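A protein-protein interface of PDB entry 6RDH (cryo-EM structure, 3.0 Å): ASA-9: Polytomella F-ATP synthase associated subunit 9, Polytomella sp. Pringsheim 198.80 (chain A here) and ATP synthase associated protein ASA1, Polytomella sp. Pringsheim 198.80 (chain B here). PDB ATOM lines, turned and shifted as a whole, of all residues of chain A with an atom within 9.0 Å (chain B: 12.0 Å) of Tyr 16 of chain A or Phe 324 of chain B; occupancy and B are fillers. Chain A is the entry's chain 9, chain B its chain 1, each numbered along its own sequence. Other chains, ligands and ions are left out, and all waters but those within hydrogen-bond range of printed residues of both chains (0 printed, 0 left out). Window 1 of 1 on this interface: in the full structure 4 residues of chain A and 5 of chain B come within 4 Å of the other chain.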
ATOM      1  N   LEU A   7      33.944   7.476 -16.063  1.00  0.00           N
ATOM      2  CA  LEU A   7      32.566   7.361 -16.516  1.00  0.00           C
ATOM      3  C   LEU A   7      31.583   7.440 -15.361  1.00  0.00           C
ATOM      4  O   LEU A   7      30.446   7.858 -15.573  1.00  0.00           O
ATOM      5  CB  LEU A   7      32.365   6.067 -17.313  1.00  0.00           C
ATOM      6  CG  LEU A   7      32.371   4.684 -16.657  1.00  0.00           C
ATOM      7  CD1 LEU A   7      31.695   3.705 -17.585  1.00  0.00           C
ATOM      8  CD2 LEU A   7      33.774   4.194 -16.368  1.00  0.00           C
ATOM      9  N   GLY A   8      32.019   7.111 -14.142  1.00  0.00           N
ATOM     10  CA  GLY A   8      31.188   7.353 -12.976  1.00  0.00           C
ATOM     11  C   GLY A   8      30.963   8.833 -12.725  1.00  0.00           C
ATOM     12  O   GLY A   8      29.835   9.268 -12.488  1.00  0.00           O
ATOM     13  N   LYS A   9      32.034   9.631 -12.805  1.00  0.00           N
ATOM     14  CA  LYS A   9      31.893  11.074 -12.614  1.00  0.00           C
ATOM     15  C   LYS A   9      31.160  11.722 -13.781  1.00  0.00           C
ATOM     16  O   LYS A   9      30.380  12.663 -13.589  1.00  0.00           O
ATOM     17  CB  LYS A   9      33.262  11.713 -12.421  1.00  0.00           C
ATOM     18  CG  LYS A   9      33.948  11.280 -11.150  1.00  0.00           C
ATOM     19  CD  LYS A   9      35.317  11.903 -11.016  1.00  0.00           C
ATOM     20  CE  LYS A   9      35.981  11.451  -9.736  1.00  0.00           C
ATOM     21  NZ  LYS A   9      37.324  12.050  -9.581  1.00  0.00           N
ATOM     22  N   ALA A  10      31.374  11.202 -14.990  1.00  0.00           N
ATOM     23  CA  ALA A  10      30.673  11.704 -16.164  1.00  0.00           C
ATOM     24  C   ALA A  10      29.185  11.405 -16.089  1.00  0.00           C
ATOM     25  O   ALA A  10      28.358  12.259 -16.426  1.00  0.00           O
ATOM     26  CB  ALA A  10      31.276  11.092 -17.425  1.00  0.00           C
ATOM     27  N   PHE A  11      28.825  10.207 -15.622  1.00  0.00           N
ATOM     28  CA  PHE A  11      27.418   9.882 -15.471  1.00  0.00           C
ATOM     29  C   PHE A  11      26.797  10.629 -14.305  1.00  0.00           C
ATOM     30  O   PHE A  11      25.608  10.943 -14.359  1.00  0.00           O
ATOM     31  CB  PHE A  11      27.218   8.379 -15.294  1.00  0.00           C
ATOM     32  CG  PHE A  11      25.777   7.982 -15.277  1.00  0.00           C
ATOM     33  CD1 PHE A  11      25.048   7.959 -16.450  1.00  0.00           C
ATOM     34  CD2 PHE A  11      25.134   7.689 -14.089  1.00  0.00           C
ATOM     35  CE1 PHE A  11      23.716   7.625 -16.441  1.00  0.00           C
ATOM     36  CE2 PHE A  11      23.802   7.363 -14.077  1.00  0.00           C
ATOM     37  CZ  PHE A  11      23.095   7.328 -15.253  1.00  0.00           C
ATOM     38  N   GLU A  12      27.572  10.921 -13.255  1.00  0.00           N
ATOM     39  CA  GLU A  12      27.060  11.755 -12.172  1.00  0.00           C
ATOM     40  C   GLU A  12      26.730  13.154 -12.670  1.00  0.00           C
ATOM     41  O   GLU A  12      25.667  13.697 -12.346  1.00  0.00           O
ATOM     42  CB  GLU A  12      28.070  11.822 -11.030  1.00  0.00           C
ATOM     43  CG  GLU A  12      27.673  12.789  -9.931  1.00  0.00           C
ATOM     44  CD  GLU A  12      28.736  12.937  -8.868  1.00  0.00           C
ATOM     45  OE1 GLU A  12      29.742  12.201  -8.929  1.00  0.00           O
ATOM     46  OE2 GLU A  12      28.568  13.795  -7.977  1.00  0.00           O
ATOM     47  N   LYS A  13      27.607  13.726 -13.501  1.00  0.00           N
ATOM     48  CA  LYS A  13      27.332  15.022 -14.120  1.00  0.00           C
ATOM     49  C   LYS A  13      26.116  14.965 -15.037  1.00  0.00           C
ATOM     50  O   LYS A  13      25.228  15.828 -14.950  1.00  0.00           O
ATOM     51  CB  LYS A  13      28.555  15.495 -14.899  1.00  0.00           C
ATOM     52  CG  LYS A  13      29.761  15.824 -14.046  1.00  0.00           C
ATOM     53  CD  LYS A  13      29.612  17.137 -13.303  1.00  0.00           C
ATOM     54  CE  LYS A  13      29.803  18.307 -14.261  1.00  0.00           C
ATOM     55  NZ  LYS A  13      29.869  19.630 -13.576  1.00  0.00           N
ATOM     56  N   TYR A  14      26.048  13.939 -15.898  1.00  0.00           N
ATOM     57  CA  TYR A  14      24.948  13.826 -16.851  1.00  0.00           C
ATOM     58  C   TYR A  14      23.615  13.600 -16.150  1.00  0.00           C
ATOM     59  O   TYR A  14      22.595  14.173 -16.546  1.00  0.00           O
ATOM     60  CB  TYR A  14      25.214  12.708 -17.859  1.00  0.00           C
ATOM     61  CG  TYR A  14      23.958  12.308 -18.597  1.00  0.00           C
ATOM     62  CD1 TYR A  14      23.353  13.176 -19.495  1.00  0.00           C
ATOM     63  CD2 TYR A  14      23.360  11.076 -18.373  1.00  0.00           C
ATOM     64  CE1 TYR A  14      22.197  12.828 -20.140  1.00  0.00           C
ATOM     65  CE2 TYR A  14      22.208  10.722 -19.020  1.00  0.00           C
ATOM     66  CZ  TYR A  14      21.633  11.598 -19.899  1.00  0.00           C
ATOM     67  OH  TYR A  14      20.480  11.235 -20.543  1.00  0.00           O
ATOM     68  N   PHE A  15      23.607  12.788 -15.098  1.00  0.00           N
ATOM     69  CA  PHE A  15      22.373  12.514 -14.384  1.00  0.00           C
ATOM     70  C   PHE A  15      21.937  13.720 -13.572  1.00  0.00           C
ATOM     71  O   PHE A  15      20.767  14.108 -13.611  1.00  0.00           O
ATOM     72  CB  PHE A  15      22.564  11.291 -13.490  1.00  0.00           C
ATOM     73  CG  PHE A  15      21.348  10.913 -12.701  1.00  0.00           C
ATOM     74  CD1 PHE A  15      21.283  11.168 -11.349  1.00  0.00           C
ATOM     75  CD2 PHE A  15      20.280  10.285 -13.305  1.00  0.00           C
ATOM     76  CE1 PHE A  15      20.175  10.824 -10.626  1.00  0.00           C
ATOM     77  CE2 PHE A  15      19.171   9.936 -12.577  1.00  0.00           C
ATOM     78  CZ  PHE A  15      19.120  10.209 -11.240  1.00  0.00           C
ATOM     79  N   TYR A  16      22.862  14.360 -12.868  1.00  0.00           N
ATOM     80  CA  TYR A  16      22.443  15.351 -11.895  1.00  0.00           C
ATOM     81  C   TYR A  16      22.279  16.738 -12.503  1.00  0.00           C
ATOM     82  O   TYR A  16      21.186  17.307 -12.445  1.00  0.00           O
ATOM     83  CB  TYR A  16      23.427  15.366 -10.728  1.00  0.00           C
ATOM     84  CG  TYR A  16      23.057  14.355  -9.681  1.00  0.00           C
ATOM     85  CD1 TYR A  16      23.957  13.384  -9.279  1.00  0.00           C
ATOM     86  CD2 TYR A  16      21.793  14.358  -9.119  1.00  0.00           C
ATOM     87  CE1 TYR A  16      23.614  12.459  -8.331  1.00  0.00           C
ATOM     88  CE2 TYR A  16      21.443  13.442  -8.175  1.00  0.00           C
ATOM     89  CZ  TYR A  16      22.357  12.496  -7.785  1.00  0.00           C
ATOM     90  OH  TYR A  16      22.005  11.573  -6.837  1.00  0.00           O
ATOM     91  N   ASP A  17      23.340  17.302 -13.092  1.00  0.00           N
ATOM     92  CA  ASP A  17      23.265  18.708 -13.466  1.00  0.00           C
ATOM     93  C   ASP A  17      23.429  18.999 -14.948  1.00  0.00           C
ATOM     94  O   ASP A  17      23.343  20.167 -15.332  1.00  0.00           O
ATOM     95  CB  ASP A  17      24.275  19.549 -12.664  1.00  0.00           C
ATOM     96  CG  ASP A  17      25.631  18.904 -12.552  1.00  0.00           C
ATOM     97  OD1 ASP A  17      25.793  17.762 -13.002  1.00  0.00           O
ATOM     98  OD2 ASP A  17      26.543  19.543 -11.996  1.00  0.00           O
ATOM     99  N   PHE A  18      23.635  17.994 -15.794  1.00  0.00           N
ATOM    100  CA  PHE A  18      23.616  18.203 -17.241  1.00  0.00           C
ATOM    101  C   PHE A  18      22.173  18.040 -17.707  1.00  0.00           C
ATOM    102  O   PHE A  18      21.802  17.075 -18.375  1.00  0.00           O
ATOM    103  CB  PHE A  18      24.550  17.219 -17.930  1.00  0.00           C
ATOM    104  CG  PHE A  18      24.992  17.620 -19.313  1.00  0.00           C
ATOM    105  CD1 PHE A  18      24.188  17.376 -20.419  1.00  0.00           C
ATOM    106  CD2 PHE A  18      26.246  18.175 -19.513  1.00  0.00           C
ATOM    107  CE1 PHE A  18      24.604  17.724 -21.685  1.00  0.00           C
ATOM    108  CE2 PHE A  18      26.668  18.525 -20.780  1.00  0.00           C
ATOM    109  CZ  PHE A  18      25.847  18.298 -21.868  1.00  0.00           C
ATOM    110  N   SER A  19      21.343  19.012 -17.351  1.00  0.00           N
ATOM    111  CA  SER A  19      19.910  18.940 -17.599  1.00  0.00           C
ATOM    112  C   SER A  19      19.550  19.678 -18.876  1.00  0.00           C
ATOM    113  O   SER A  19      19.866  20.860 -19.020  1.00  0.00           O
ATOM    114  CB  SER A  19      19.122  19.533 -16.436  1.00  0.00           C
ATOM    115  OG  SER A  19      17.741  19.547 -16.743  1.00  0.00           O
ATOM    116  N   ALA A  20      18.857  18.994 -19.779  1.00  0.00           N
ATOM    117  CA  ALA A  20      18.363  19.599 -21.003  1.00  0.00           C
ATOM    118  C   ALA A  20      16.964  20.171 -20.851  1.00  0.00           C
ATOM    119  O   ALA A  20      16.318  20.473 -21.857  1.00  0.00           O
ATOM    120  CB  ALA A  20      18.382  18.585 -22.145  1.00  0.00           C
ATOM    121  N   LYS A  33       7.882  20.591 -14.628  1.00  0.00           N
ATOM    122  CA  LYS A  33       8.844  19.545 -14.933  1.00  0.00           C
ATOM    123  C   LYS A  33       8.235  18.158 -14.842  1.00  0.00           C
ATOM    124  O   LYS A  33       8.756  17.224 -15.456  1.00  0.00           O
ATOM    125  CB  LYS A  33      10.055  19.628 -14.001  1.00  0.00           C
ATOM    126  CG  LYS A  33      11.324  19.113 -14.639  1.00  0.00           C
ATOM    127  CD  LYS A  33      12.548  19.430 -13.817  1.00  0.00           C
ATOM    128  CE  LYS A  33      13.791  18.897 -14.502  1.00  0.00           C
ATOM    129  NZ  LYS A  33      15.031  19.253 -13.768  1.00  0.00           N
ATOM    130  N   LEU B 315      24.507  11.943   9.677  1.00  0.00           N
ATOM    131  CA  LEU B 315      23.910  11.209   8.573  1.00  0.00           C
ATOM    132  C   LEU B 315      24.486  11.632   7.234  1.00  0.00           C
ATOM    133  O   LEU B 315      24.525  10.827   6.303  1.00  0.00           O
ATOM    134  CB  LEU B 315      22.402  11.416   8.553  1.00  0.00           C
ATOM    135  CG  LEU B 315      21.510  10.337   9.136  1.00  0.00           C
ATOM    136  CD1 LEU B 315      20.088  10.682   8.847  1.00  0.00           C
ATOM    137  CD2 LEU B 315      21.850   9.009   8.542  1.00  0.00           C
ATOM    138  N   ASN B 316      24.909  12.890   7.108  1.00  0.00           N
ATOM    139  CA  ASN B 316      25.496  13.363   5.860  1.00  0.00           C
ATOM    140  C   ASN B 316      26.824  12.693   5.564  1.00  0.00           C
ATOM    141  O   ASN B 316      27.182  12.523   4.397  1.00  0.00           O
ATOM    142  CB  ASN B 316      25.683  14.868   5.913  1.00  0.00           C
ATOM    143  CG  ASN B 316      24.419  15.602   5.645  1.00  0.00           C
ATOM    144  OD1 ASN B 316      24.053  16.529   6.358  1.00  0.00           O
ATOM    145  ND2 ASN B 316      23.729  15.192   4.609  1.00  0.00           N
ATOM    146  N   SER B 318      27.483   9.599   6.473  1.00  0.00           N
ATOM    147  CA  SER B 318      27.252   8.170   6.460  1.00  0.00           C
ATOM    148  C   SER B 318      27.492   7.622   5.057  1.00  0.00           C
ATOM    149  O   SER B 318      27.538   8.385   4.093  1.00  0.00           O
ATOM    150  CB  SER B 318      25.826   7.887   6.916  1.00  0.00           C
ATOM    151  OG  SER B 318      24.905   8.577   6.105  1.00  0.00           O
ATOM    152  N   PRO B 319      27.668   6.303   4.909  1.00  0.00           N
ATOM    153  CA  PRO B 319      27.797   5.736   3.560  1.00  0.00           C
ATOM    154  C   PRO B 319      26.542   5.841   2.720  1.00  0.00           C
ATOM    155  O   PRO B 319      26.621   5.654   1.503  1.00  0.00           O
ATOM    156  CB  PRO B 319      28.140   4.272   3.830  1.00  0.00           C
ATOM    157  CG  PRO B 319      28.755   4.271   5.138  1.00  0.00           C
ATOM    158  CD  PRO B 319      28.072   5.320   5.929  1.00  0.00           C
ATOM    159  N   ALA B 320      25.397   6.133   3.315  1.00  0.00           N
ATOM    160  CA  ALA B 320      24.165   6.209   2.555  1.00  0.00           C
ATOM    161  C   ALA B 320      24.070   7.473   1.729  1.00  0.00           C
ATOM    162  O   ALA B 320      23.359   7.488   0.726  1.00  0.00           O
ATOM    163  CB  ALA B 320      22.977   6.132   3.498  1.00  0.00           C
ATOM    164  N   PHE B 321      24.747   8.538   2.133  1.00  0.00           N
ATOM    165  CA  PHE B 321      24.679   9.802   1.423  1.00  0.00           C
ATOM    166  C   PHE B 321      25.878  10.031   0.525  1.00  0.00           C
ATOM    167  O   PHE B 321      25.946  11.057  -0.147  1.00  0.00           O
ATOM    168  CB  PHE B 321      24.517  10.951   2.410  1.00  0.00           C
ATOM    169  CG  PHE B 321      23.104  11.171   2.821  1.00  0.00           C
ATOM    170  CD1 PHE B 321      22.339  12.129   2.203  1.00  0.00           C
ATOM    171  CD2 PHE B 321      22.528  10.399   3.801  1.00  0.00           C
ATOM    172  CE1 PHE B 321      21.039  12.320   2.565  1.00  0.00           C
ATOM    173  CE2 PHE B 321      21.226  10.594   4.161  1.00  0.00           C
ATOM    174  CZ  PHE B 321      20.484  11.553   3.539  1.00  0.00           C
ATOM    175  N   SER B 322      26.822   9.105   0.505  1.00  0.00           N
ATOM    176  CA  SER B 322      27.832   9.047  -0.535  1.00  0.00           C
ATOM    177  C   SER B 322      27.445   8.101  -1.658  1.00  0.00           C
ATOM    178  O   SER B 322      28.231   7.911  -2.587  1.00  0.00           O
ATOM    179  CB  SER B 322      29.173   8.618   0.057  1.00  0.00           C
ATOM    180  OG  SER B 322      29.565   9.496   1.095  1.00  0.00           O
ATOM    181  N   SER B 323      26.266   7.494  -1.589  1.00  0.00           N
ATOM    182  CA  SER B 323      25.774   6.688  -2.688  1.00  0.00           C
ATOM    183  C   SER B 323      25.248   7.594  -3.784  1.00  0.00           C
ATOM    184  O   SER B 323      25.120   8.802  -3.609  1.00  0.00           O
ATOM    185  CB  SER B 323      24.674   5.749  -2.232  1.00  0.00           C
ATOM    186  OG  SER B 323      23.514   6.490  -1.945  1.00  0.00           O
ATOM    187  N   PHE B 324      24.897   6.988  -4.916  1.00  0.00           N
ATOM    188  CA  PHE B 324      24.658   7.767  -6.122  1.00  0.00           C
ATOM    189  C   PHE B 324      23.348   8.537  -6.052  1.00  0.00           C
ATOM    190  O   PHE B 324      23.313   9.738  -6.332  1.00  0.00           O
ATOM    191  CB  PHE B 324      24.673   6.857  -7.340  1.00  0.00           C
ATOM    192  CG  PHE B 324      24.468   7.587  -8.618  1.00  0.00           C
ATOM    193  CD1 PHE B 324      25.482   8.355  -9.148  1.00  0.00           C
ATOM    194  CD2 PHE B 324      23.258   7.527  -9.281  1.00  0.00           C
ATOM    195  CE1 PHE B 324      25.300   9.039 -10.307  1.00  0.00           C
ATOM    196  CE2 PHE B 324      23.074   8.211 -10.441  1.00  0.00           C
ATOM    197  CZ  PHE B 324      24.097   8.968 -10.956  1.00  0.00           C
ATOM    198  N   LEU B 325      22.262   7.873  -5.668  1.00  0.00           N
ATOM    199  CA  LEU B 325      20.952   8.508  -5.694  1.00  0.00           C
ATOM    200  C   LEU B 325      20.747   9.514  -4.573  1.00  0.00           C
ATOM    201  O   LEU B 325      19.757  10.245  -4.602  1.00  0.00           O
ATOM    202  CB  LEU B 325      19.863   7.446  -5.624  1.00  0.00           C
ATOM    203  CG  LEU B 325      19.916   6.381  -6.714  1.00  0.00           C
ATOM    204  CD1 LEU B 325      18.854   5.344  -6.481  1.00  0.00           C
ATOM    205  CD2 LEU B 325      19.739   7.020  -8.066  1.00  0.00           C
ATOM    206  N   LEU B 326      21.651   9.578  -3.604  1.00  0.00           N
ATOM    207  CA  LEU B 326      21.541  10.487  -2.472  1.00  0.00           C
ATOM    208  C   LEU B 326      22.767  11.372  -2.358  1.00  0.00           C
ATOM    209  O   LEU B 326      23.099  11.842  -1.274  1.00  0.00           O
ATOM    210  CB  LEU B 326      21.345   9.712  -1.175  1.00  0.00           C
ATOM    211  CG  LEU B 326      20.003   9.050  -0.957  1.00  0.00           C
ATOM    212  CD1 LEU B 326      20.162   8.010   0.087  1.00  0.00           C
ATOM    213  CD2 LEU B 326      19.036  10.075  -0.508  1.00  0.00           C
ATOM    214  N   LYS B 327      23.451  11.604  -3.472  1.00  0.00           N
ATOM    215  CA  LYS B 327      24.742  12.272  -3.427  1.00  0.00           C
ATOM    216  C   LYS B 327      24.598  13.784  -3.377  1.00  0.00           C
ATOM    217  O   LYS B 327      25.415  14.455  -2.742  1.00  0.00           O
ATOM    218  CB  LYS B 327      25.564  11.838  -4.633  1.00  0.00           C
ATOM    219  CG  LYS B 327      27.030  12.085  -4.522  1.00  0.00           C
ATOM    220  CD  LYS B 327      27.727  11.519  -5.732  1.00  0.00           C
ATOM    221  CE  LYS B 327      27.743  10.014  -5.684  1.00  0.00           C
ATOM    222  NZ  LYS B 327      28.510   9.436  -6.815  1.00  0.00           N
ATOM    223  N   ARG B 328      23.577  14.336  -4.020  1.00  0.00           N
ATOM    224  CA  ARG B 328      23.312  15.767  -3.984  1.00  0.00           C
ATOM    225  C   ARG B 328      22.426  16.182  -2.824  1.00  0.00           C
ATOM    226  O   ARG B 328      22.307  17.379  -2.557  1.00  0.00           O
ATOM    227  CB  ARG B 328      22.652  16.218  -5.286  1.00  0.00           C
ATOM    228  CG  ARG B 328      23.519  16.077  -6.512  1.00  0.00           C
ATOM    229  CD  ARG B 328      24.481  17.222  -6.670  1.00  0.00           C
ATOM    230  NE  ARG B 328      25.171  17.166  -7.950  1.00  0.00           N
ATOM    231  CZ  ARG B 328      26.292  16.485  -8.154  1.00  0.00           C
ATOM    232  NH1 ARG B 328      26.839  15.801  -7.160  1.00  0.00           N
ATOM    233  NH2 ARG B 328      26.866  16.489  -9.345  1.00  0.00           N
ATOM    234  N   GLU B 329      21.800  15.235  -2.139  1.00  0.00           N
ATOM    235  CA  GLU B 329      20.831  15.544  -1.103  1.00  0.00           C
ATOM    236  C   GLU B 329      21.527  15.822   0.221  1.00  0.00           C
ATOM    237  O   GLU B 329      22.720  15.569   0.397  1.00  0.00           O
ATOM    238  CB  GLU B 329      19.835  14.401  -0.942  1.00  0.00           C
ATOM    239  CG  GLU B 329      19.029  14.099  -2.180  1.00  0.00           C
ATOM    240  CD  GLU B 329      18.364  15.326  -2.759  1.00  0.00           C
ATOM    241  OE1 GLU B 329      18.587  15.618  -3.951  1.00  0.00           O
ATOM    242  OE2 GLU B 329      17.620  16.006  -2.024  1.00  0.00           O
ATOM    243  N   LYS B 330      20.764  16.367   1.159  1.00  0.00           N
ATOM    244  CA  LYS B 330      21.258  16.646   2.495  1.00  0.00           C
ATOM    245  C   LYS B 330      20.255  16.131   3.511  1.00  0.00           C
ATOM    246  O   LYS B 330      19.045  16.265   3.323  1.00  0.00           O
ATOM    247  CB  LYS B 330      21.499  18.140   2.696  1.00  0.00           C
ATOM    248  CG  LYS B 330      22.710  18.666   1.955  1.00  0.00           C
ATOM    249  CD  LYS B 330      23.958  17.926   2.378  1.00  0.00           C
ATOM    250  CE  LYS B 330      25.136  18.260   1.492  1.00  0.00           C
ATOM    251  NZ  LYS B 330      26.332  17.460   1.867  1.00  0.00           N
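Among the printed residues, merely in contact across the chains: Phe 11 of chain A with Phe 324 of chain B, Tyr 16 of chain A with Arg 328 of chain B, Phe 15 of chain A with Phe 324 of chain B, Tyr 16 of chain A with Lys 327 of chain B, Glu 12 of chain A with Phe 324 of chain B and Tyr 16 of chain A with Leu 326 of chain B.
Of the 15 printed residues of chain B, 5 touch a printed residue of chain A. Hydrophobic or aromatic side chains of chain B that line the printed part of chain A: Phe 324. Printed residues of chain A that touch a printed residue of chain B: Phe 11, Glu 12, Phe 15 and Tyr 16. Among the printed residues, 10 pairs touch across the chains. Among the printed residues, Asp or Glu carboxylates within 4 Å of a Lys or Arg side-chain nitrogen of the other chain: Glu 12 of chain A with Lys 327 of chain B (3.7 Å) and Glu 12 of chain A with Arg 328 of chain B (2.8 Å).
Of the printed residues of chain B, Phe 11 of chain A touches Phe 324 (3.5 Å). Of chain B, only Phe 324 (3.7 Å), Lys 327 (3.3 Å) and Arg 328 (2.8 Å) come within 4 Å of Glu 12 of chain A. Phe 15 of chain A touches one residue of chain B. No residue of chain B comes within 4 Å of Ser 19 of chain A. No residue of chain A comes within 4 Å of Ser 323 of chain B. Phe 324 of chain B touches just these residues of chain A: Phe 11 (3.5 Å), Glu 12 (3.7 Å), Phe 15 (3.6 Å) and Tyr 16 (2.3 Å). Of the printed residues of chain A, Leu 325 of chain B touches Tyr 16 (3.3 Å). Of the printed residues of chain A, Leu 326 of chain B touches Tyr 16. Printed residues of chain A within 4 Å of Lys 327 of chain B: Glu 12 and Tyr 16. Printed residues of chain A within 4 Å of Arg 328 of chain B: Glu 12 (2.8 Å) and Tyr 16 (3.6 Å). The nearest residue of chain B that does not touch Tyr 16 of chain A is Ser 323 of chain B (5.3 Å). The nearest residue of chain A that does not touch Phe 324 of chain B is Gly 8 of chain A (5.0 Å).
The side-chain carboxylate (OE1) of Glu 12 of chain A is in salt-bridge range of the side-chain amino group (NZ) of Lys 327 of chain B, 3.7 Å away. OE2 of Glu 12 of chain A lies within salt-bridge range of NH1 of Arg 328 of chain B, 2.8 Å away. The side-chain hydroxyl (OH) of Tyr 16 of chain A sits close to the backbone carbonyl oxygen (O) of Leu 325 of chain B (3.4 Å). The side-chain hydroxyl (OH) of Tyr 16 of chain A sits close to the backbone carbonyl oxygen (O) of Phe 324 of chain B (2.3 Å).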
